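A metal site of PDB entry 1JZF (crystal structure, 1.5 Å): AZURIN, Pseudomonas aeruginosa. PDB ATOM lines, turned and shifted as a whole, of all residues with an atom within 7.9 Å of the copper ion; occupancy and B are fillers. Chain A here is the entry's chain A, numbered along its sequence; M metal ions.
ND1 of His 117 lies close to O of Gly 45. A ring nitrogen (NE2) of His 46 is in hydrogen-bond range of the backbone carbonyl oxygen (O) of Asn 10 (2.8 Å). The backbone NH (N) of Phe 114 sits close to the side-chain sulfur (SG) of Cys 112 (3.4 Å). The side-chain sulfur (SD) of Met 44 lies close to a ring nitrogen (NE2) of His 117. The backbone carbonyl oxygen of Met 121 is in hydrogen-bond range of the backbone NH of Cys 112 (3.2 Å). O of His 46 is in hydrogen-bond range of N of Ile 87 (2.8 Å). The side-chain sulfur of Cys 112 lies close to the side-chain amide oxygen of Asn 47. The side-chain sulfur (SG) of Cys 112 lies close to the backbone carbonyl oxygen (O) of Gly 45, at 3.6 Å.
The copper ion is bound by ND1 of His 46, ND1 of His 117 and SG of Cys 112. The copper ion has three donor atoms within binding distance. Slightly farther from the copper ion lies O of Gly 45 (2.6 Å).
Phe 114 touches the copper ion. Met 121 touches the copper ion (SD to CU, 3.3 Å). Of the 25 residues printed, 6 come within 4 Å of the copper ion. The nearest printed residue that does not touch the copper ion is Asn 47 (4.6 Å).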
ATOM      1  N   GLY A   9       2.777  26.572  12.593  1.00  0.00           N
ATOM      2  CA  GLY A   9       1.494  27.246  12.546  1.00  0.00           C
ATOM      3  C   GLY A   9       1.874  28.719  12.463  1.00  0.00           C
ATOM      4  O   GLY A   9       2.572  29.212  13.350  1.00  0.00           O
ATOM      5  N   ASN A  10       1.418  29.424  11.434  1.00  0.00           N
ATOM      6  CA  ASN A  10       1.782  30.821  11.246  1.00  0.00           C
ATOM      7  C   ASN A  10       0.666  31.880  11.388  1.00  0.00           C
ATOM      8  O   ASN A  10      -0.440  31.569  11.814  1.00  0.00           O
ATOM      9  CB  ASN A  10       2.497  30.988   9.903  1.00  0.00           C
ATOM     10  CG  ASN A  10       1.610  30.628   8.719  1.00  0.00           C
ATOM     11  OD1 ASN A  10       0.382  30.619   8.820  1.00  0.00           O
ATOM     12  ND2 ASN A  10       2.240  30.337   7.587  1.00  0.00           N
ATOM     13  N   MET A  13      -2.775  31.701   9.515  1.00  0.00           N
ATOM     14  CA  MET A  13      -3.694  30.686  10.041  1.00  0.00           C
ATOM     15  C   MET A  13      -3.602  29.387   9.236  1.00  0.00           C
ATOM     16  O   MET A  13      -4.614  28.827   8.803  1.00  0.00           O
ATOM     17  CB  MET A  13      -5.127  31.252  10.027  1.00  0.00           C
ATOM     18  CG  MET A  13      -6.103  30.526  10.937  1.00  0.00           C
ATOM     19  SD  MET A  13      -7.743  31.240  10.752  1.00  0.00           S
ATOM     20  CE  MET A  13      -8.211  30.499   9.188  1.00  0.00           C
ATOM     21  N   GLN A  14      -2.377  28.910   9.029  1.00  0.00           N
ATOM     22  CA  GLN A  14      -2.128  27.685   8.279  1.00  0.00           C
ATOM     23  C   GLN A  14      -1.034  26.802   8.872  1.00  0.00           C
ATOM     24  O   GLN A  14      -0.084  27.296   9.473  1.00  0.00           O
ATOM     25  CB  GLN A  14      -1.714  28.008   6.836  1.00  0.00           C
ATOM     26  CG  GLN A  14      -2.760  28.725   6.002  1.00  0.00           C
ATOM     27  CD  GLN A  14      -2.259  29.081   4.604  1.00  0.00           C
ATOM     28  OE1 GLN A  14      -2.699  28.502   3.609  1.00  0.00           O
ATOM     29  NE2 GLN A  14      -1.342  30.033   4.538  1.00  0.00           N
ATOM     30  N   PHE A  15      -1.220  25.486   8.754  1.00  0.00           N
ATOM     31  CA  PHE A  15      -0.224  24.511   9.186  1.00  0.00           C
ATOM     32  C   PHE A  15       0.584  24.283   7.912  1.00  0.00           C
ATOM     33  O   PHE A  15       0.085  24.540   6.809  1.00  0.00           O
ATOM     34  CB  PHE A  15      -0.890  23.173   9.566  1.00  0.00           C
ATOM     35  CG  PHE A  15      -1.420  23.127  10.977  1.00  0.00           C
ATOM     36  CD1 PHE A  15      -0.641  23.510  12.052  1.00  0.00           C
ATOM     37  CD2 PHE A  15      -2.703  22.628  11.220  1.00  0.00           C
ATOM     38  CE1 PHE A  15      -1.122  23.393  13.365  1.00  0.00           C
ATOM     39  CE2 PHE A  15      -3.191  22.518  12.519  1.00  0.00           C
ATOM     40  CZ  PHE A  15      -2.399  22.904  13.589  1.00  0.00           C
ATOM     41  N   LEU A  33       5.612  21.080  17.240  1.00  0.00           N
ATOM     42  CA  LEU A  33       4.940  22.280  16.754  1.00  0.00           C
ATOM     43  C   LEU A  33       5.670  23.575  17.113  1.00  0.00           C
ATOM     44  O   LEU A  33       6.175  23.720  18.217  1.00  0.00           O
ATOM     45  CB  LEU A  33       3.516  22.346  17.309  1.00  0.00           C
ATOM     46  CG  LEU A  33       2.648  23.542  16.888  1.00  0.00           C
ATOM     47  CD1 LEU A  33       2.274  23.409  15.423  1.00  0.00           C
ATOM     48  CD2 LEU A  33       1.401  23.610  17.746  1.00  0.00           C
ATOM     49  N   HIS A  35       5.663  28.124  16.154  1.00  0.00           N
ATOM     50  CA  HIS A  35       4.888  29.252  15.648  1.00  0.00           C
ATOM     51  C   HIS A  35       5.816  30.344  15.112  1.00  0.00           C
ATOM     52  O   HIS A  35       6.310  31.189  15.872  1.00  0.00           O
ATOM     53  CB  HIS A  35       4.016  29.805  16.783  1.00  0.00           C
ATOM     54  CG  HIS A  35       2.931  30.745  16.320  1.00  0.00           C
ATOM     55  ND1 HIS A  35       3.152  31.734  15.388  1.00  0.00           N
ATOM     56  CD2 HIS A  35       1.647  30.856  16.703  1.00  0.00           C
ATOM     57  CE1 HIS A  35       2.037  32.417  15.207  1.00  0.00           C
ATOM     58  NE2 HIS A  35       1.101  31.900  16.000  1.00  0.00           N
ATOM     59  N   LYS A  41      -0.568  34.360  21.307  1.00  0.00           N
ATOM     60  CA  LYS A  41      -1.525  33.249  21.356  1.00  0.00           C
ATOM     61  C   LYS A  41      -2.987  33.614  21.594  1.00  0.00           C
ATOM     62  O   LYS A  41      -3.881  32.814  21.311  1.00  0.00           O
ATOM     63  CB  LYS A  41      -1.074  32.172  22.355  1.00  0.00           C
ATOM     64  CG  LYS A  41      -1.278  32.501  23.824  1.00  0.00           C
ATOM     65  CD  LYS A  41      -0.897  31.289  24.670  1.00  0.00           C
ATOM     66  CE  LYS A  41      -1.193  31.519  26.144  1.00  0.00           C
ATOM     67  NZ  LYS A  41      -0.735  30.367  26.974  1.00  0.00           N
ATOM     68  N   VAL A  43      -4.593  35.945  20.011  1.00  0.00           N
ATOM     69  CA  VAL A  43      -5.183  36.372  18.747  1.00  0.00           C
ATOM     70  C   VAL A  43      -4.899  35.382  17.608  1.00  0.00           C
ATOM     71  O   VAL A  43      -5.712  35.254  16.687  1.00  0.00           O
ATOM     72  CB  VAL A  43      -4.691  37.784  18.314  1.00  0.00           C
ATOM     73  CG1 VAL A  43      -4.992  38.810  19.400  1.00  0.00           C
ATOM     74  CG2 VAL A  43      -3.202  37.762  18.001  1.00  0.00           C
ATOM     75  N   MET A  44      -3.769  34.704  17.689  1.00  0.00           N
ATOM     76  CA  MET A  44      -3.374  33.729  16.660  1.00  0.00           C
ATOM     77  C   MET A  44      -2.724  32.509  17.314  1.00  0.00           C
ATOM     78  O   MET A  44      -1.700  31.999  16.838  1.00  0.00           O
ATOM     79  CB  MET A  44      -2.417  34.401  15.656  1.00  0.00           C
ATOM     80  CG  MET A  44      -2.064  33.582  14.416  1.00  0.00           C
ATOM     81  SD  MET A  44      -3.489  33.143  13.399  1.00  0.00           S
ATOM     82  CE  MET A  44      -3.948  34.745  12.732  1.00  0.00           C
ATOM     83  N   GLY A  45      -3.312  32.048  18.403  1.00  0.00           N
ATOM     84  CA  GLY A  45      -2.790  30.887  19.107  1.00  0.00           C
ATOM     85  C   GLY A  45      -3.012  29.607  18.332  1.00  0.00           C
ATOM     86  O   GLY A  45      -4.047  29.449  17.671  1.00  0.00           O
ATOM     87  N   HIS A  46      -2.042  28.709  18.384  1.00  0.00           N
ATOM     88  CA  HIS A  46      -2.125  27.434  17.683  1.00  0.00           C
ATOM     89  C   HIS A  46      -1.768  26.242  18.545  1.00  0.00           C
ATOM     90  O   HIS A  46      -0.825  26.284  19.338  1.00  0.00           O
ATOM     91  CB  HIS A  46      -1.186  27.411  16.475  1.00  0.00           C
ATOM     92  CG  HIS A  46      -1.469  28.448  15.441  1.00  0.00           C
ATOM     93  ND1 HIS A  46      -2.747  28.784  15.037  1.00  0.00           N
ATOM     94  CD2 HIS A  46      -0.637  29.228  14.717  1.00  0.00           C
ATOM     95  CE1 HIS A  46      -2.680  29.708  14.104  1.00  0.00           C
ATOM     96  NE2 HIS A  46      -1.413  30.004  13.887  1.00  0.00           N
ATOM     97  N   ASN A  47      -2.543  25.176  18.391  1.00  0.00           N
ATOM     98  CA  ASN A  47      -2.272  23.920  19.084  1.00  0.00           C
ATOM     99  C   ASN A  47      -2.475  22.816  18.051  1.00  0.00           C
ATOM    100  O   ASN A  47      -3.037  23.049  16.987  1.00  0.00           O
ATOM    101  CB  ASN A  47      -3.163  23.712  20.334  1.00  0.00           C
ATOM    102  CG  ASN A  47      -4.651  23.759  20.034  1.00  0.00           C
ATOM    103  OD1 ASN A  47      -5.082  23.802  18.878  1.00  0.00           O
ATOM    104  ND2 ASN A  47      -5.463  23.742  21.087  1.00  0.00           N
ATOM    105  N   TRP A  48      -1.892  21.651  18.324  1.00  0.00           N
ATOM    106  CA  TRP A  48      -2.015  20.510  17.437  1.00  0.00           C
ATOM    107  C   TRP A  48      -2.803  19.489  18.244  1.00  0.00           C
ATOM    108  O   TRP A  48      -2.306  18.943  19.233  1.00  0.00           O
ATOM    109  CB  TRP A  48      -0.629  19.969  17.058  1.00  0.00           C
ATOM    110  CG  TRP A  48      -0.670  18.867  16.050  1.00  0.00           C
ATOM    111  CD1 TRP A  48      -0.655  18.996  14.683  1.00  0.00           C
ATOM    112  CD2 TRP A  48      -0.759  17.462  16.316  1.00  0.00           C
ATOM    113  NE1 TRP A  48      -0.714  17.761  14.094  1.00  0.00           N
ATOM    114  CE2 TRP A  48      -0.776  16.795  15.063  1.00  0.00           C
ATOM    115  CE3 TRP A  48      -0.801  16.699  17.491  1.00  0.00           C
ATOM    116  CZ2 TRP A  48      -0.860  15.412  14.964  1.00  0.00           C
ATOM    117  CZ3 TRP A  48      -0.886  15.311  17.384  1.00  0.00           C
ATOM    118  CH2 TRP A  48      -0.910  14.680  16.123  1.00  0.00           C
ATOM    119  N   LEU A  86      -1.393  25.247  23.592  1.00  0.00           N
ATOM    120  CA  LEU A  86      -1.660  26.361  22.686  1.00  0.00           C
ATOM    121  C   LEU A  86      -0.446  27.282  22.753  1.00  0.00           C
ATOM    122  O   LEU A  86      -0.044  27.715  23.828  1.00  0.00           O
ATOM    123  CB  LEU A  86      -2.910  27.118  23.111  1.00  0.00           C
ATOM    124  CG  LEU A  86      -3.474  28.155  22.135  1.00  0.00           C
ATOM    125  CD1 LEU A  86      -4.237  27.455  21.029  1.00  0.00           C
ATOM    126  CD2 LEU A  86      -4.389  29.099  22.877  1.00  0.00           C
ATOM    127  N   ILE A  87       0.149  27.565  21.590  1.00  0.00           N
ATOM    128  CA  ILE A  87       1.328  28.417  21.551  1.00  0.00           C
ATOM    129  C   ILE A  87       1.161  29.653  20.660  1.00  0.00           C
ATOM    130  O   ILE A  87       0.324  29.685  19.757  1.00  0.00           O
ATOM    131  CB  ILE A  87       2.580  27.635  21.069  1.00  0.00           C
ATOM    132  CG1 ILE A  87       2.394  27.161  19.622  1.00  0.00           C
ATOM    133  CG2 ILE A  87       2.845  26.461  21.998  1.00  0.00           C
ATOM    134  CD1 ILE A  87       3.646  26.565  19.021  1.00  0.00           C
ATOM    135  N   PHE A 111      -5.835  19.134  14.128  1.00  0.00           N
ATOM    136  CA  PHE A 111      -6.375  20.470  13.912  1.00  0.00           C
ATOM    137  C   PHE A 111      -6.072  21.399  15.084  1.00  0.00           C
ATOM    138  O   PHE A 111      -5.657  20.949  16.151  1.00  0.00           O
ATOM    139  CB  PHE A 111      -7.898  20.379  13.745  1.00  0.00           C
ATOM    140  CG  PHE A 111      -8.569  19.506  14.772  1.00  0.00           C
ATOM    141  CD1 PHE A 111      -8.751  18.139  14.542  1.00  0.00           C
ATOM    142  CD2 PHE A 111      -8.984  20.025  15.998  1.00  0.00           C
ATOM    143  CE1 PHE A 111      -9.317  17.312  15.509  1.00  0.00           C
ATOM    144  CE2 PHE A 111      -9.558  19.206  16.974  1.00  0.00           C
ATOM    145  CZ  PHE A 111      -9.726  17.847  16.725  1.00  0.00           C
ATOM    146  N   CYS A 112      -6.275  22.689  14.850  1.00  0.00           N
ATOM    147  CA  CYS A 112      -6.088  23.698  15.882  1.00  0.00           C
ATOM    148  C   CYS A 112      -7.483  24.029  16.396  1.00  0.00           C
ATOM    149  O   CYS A 112      -8.421  24.167  15.592  1.00  0.00           O
ATOM    150  CB  CYS A 112      -5.459  24.956  15.299  1.00  0.00           C
ATOM    151  SG  CYS A 112      -5.343  26.316  16.495  1.00  0.00           S
ATOM    152  N   THR A 113      -7.647  24.150  17.707  1.00  0.00           N
ATOM    153  CA  THR A 113      -8.945  24.458  18.285  1.00  0.00           C
ATOM    154  C   THR A 113      -9.185  25.932  18.631  1.00  0.00           C
ATOM    155  O   THR A 113     -10.200  26.253  19.249  1.00  0.00           O
ATOM    156  CB  THR A 113      -9.247  23.579  19.509  1.00  0.00           C
ATOM    157  OG1 THR A 113      -8.276  23.815  20.536  1.00  0.00           O
ATOM    158  CG2 THR A 113      -9.233  22.099  19.130  1.00  0.00           C
ATOM    159  N   PHE A 114      -8.252  26.797  18.271  1.00  0.00           N
ATOM    160  CA  PHE A 114      -8.433  28.226  18.527  1.00  0.00           C
ATOM    161  C   PHE A 114      -9.638  28.612  17.669  1.00  0.00           C
ATOM    162  O   PHE A 114      -9.746  28.187  16.517  1.00  0.00           O
ATOM    163  CB  PHE A 114      -7.194  29.018  18.089  1.00  0.00           C
ATOM    164  CG  PHE A 114      -7.255  30.485  18.438  1.00  0.00           C
ATOM    165  CD1 PHE A 114      -7.931  31.382  17.624  1.00  0.00           C
ATOM    166  CD2 PHE A 114      -6.659  30.952  19.607  1.00  0.00           C
ATOM    167  CE1 PHE A 114      -8.015  32.731  17.952  1.00  0.00           C
ATOM    168  CE2 PHE A 114      -6.733  32.302  19.944  1.00  0.00           C
ATOM    169  CZ  PHE A 114      -7.410  33.194  19.121  1.00  0.00           C
ATOM    170  N   PRO A 115     -10.564  29.408  18.217  1.00  0.00           N
ATOM    171  CA  PRO A 115     -11.775  29.844  17.508  1.00  0.00           C
ATOM    172  C   PRO A 115     -11.619  30.192  16.021  1.00  0.00           C
ATOM    173  O   PRO A 115     -10.862  31.101  15.659  1.00  0.00           O
ATOM    174  CB  PRO A 115     -12.228  31.044  18.325  1.00  0.00           C
ATOM    175  CG  PRO A 115     -11.913  30.605  19.711  1.00  0.00           C
ATOM    176  CD  PRO A 115     -10.517  30.018  19.556  1.00  0.00           C
ATOM    177  N   GLY A 116     -12.306  29.424  15.185  1.00  0.00           N
ATOM    178  CA  GLY A 116     -12.291  29.634  13.748  1.00  0.00           C
ATOM    179  C   GLY A 116     -11.141  29.041  12.954  1.00  0.00           C
ATOM    180  O   GLY A 116     -11.254  28.850  11.751  1.00  0.00           O
ATOM    181  N   HIS A 117     -10.034  28.725  13.628  1.00  0.00           N
ATOM    182  CA  HIS A 117      -8.854  28.189  12.960  1.00  0.00           C
ATOM    183  C   HIS A 117      -8.975  26.869  12.223  1.00  0.00           C
ATOM    184  O   HIS A 117      -8.380  26.713  11.160  1.00  0.00           O
ATOM    185  CB  HIS A 117      -7.674  28.132  13.938  1.00  0.00           C
ATOM    186  CG  HIS A 117      -7.115  29.482  14.277  1.00  0.00           C
ATOM    187  ND1 HIS A 117      -5.871  29.650  14.830  1.00  0.00           N
ATOM    188  CD2 HIS A 117      -7.626  30.731  14.116  1.00  0.00           C
ATOM    189  CE1 HIS A 117      -5.632  30.940  14.999  1.00  0.00           C
ATOM    190  NE2 HIS A 117      -6.682  31.614  14.576  1.00  0.00           N
ATOM    191  N   SER A 118      -9.770  25.925  12.740  1.00  0.00           N
ATOM    192  CA  SER A 118      -9.921  24.615  12.097  1.00  0.00           C
ATOM    193  C   SER A 118     -10.497  24.686  10.684  1.00  0.00           C
ATOM    194  O   SER A 118     -10.480  23.693   9.953  1.00  0.00           O
ATOM    195  CB  SER A 118     -10.739  23.660  12.966  1.00  0.00           C
ATOM    196  OG  SER A 118     -12.114  23.987  12.950  1.00  0.00           O
ATOM    197  N   MET A 121      -6.892  25.227   9.408  1.00  0.00           N
ATOM    198  CA  MET A 121      -5.920  24.455  10.172  1.00  0.00           C
ATOM    199  C   MET A 121      -6.380  23.068  10.585  1.00  0.00           C
ATOM    200  O   MET A 121      -6.778  22.852  11.740  1.00  0.00           O
ATOM    201  CB  MET A 121      -5.429  25.260  11.367  1.00  0.00           C
ATOM    202  CG  MET A 121      -4.821  26.584  10.948  1.00  0.00           C
ATOM    203  SD  MET A 121      -4.079  27.520  12.286  1.00  0.00           S
ATOM    204  CE  MET A 121      -2.564  26.597  12.499  1.00  0.00           C
HETATM  205 CU    CU M   1      -4.608  28.130  15.498  1.00  0.00          CU
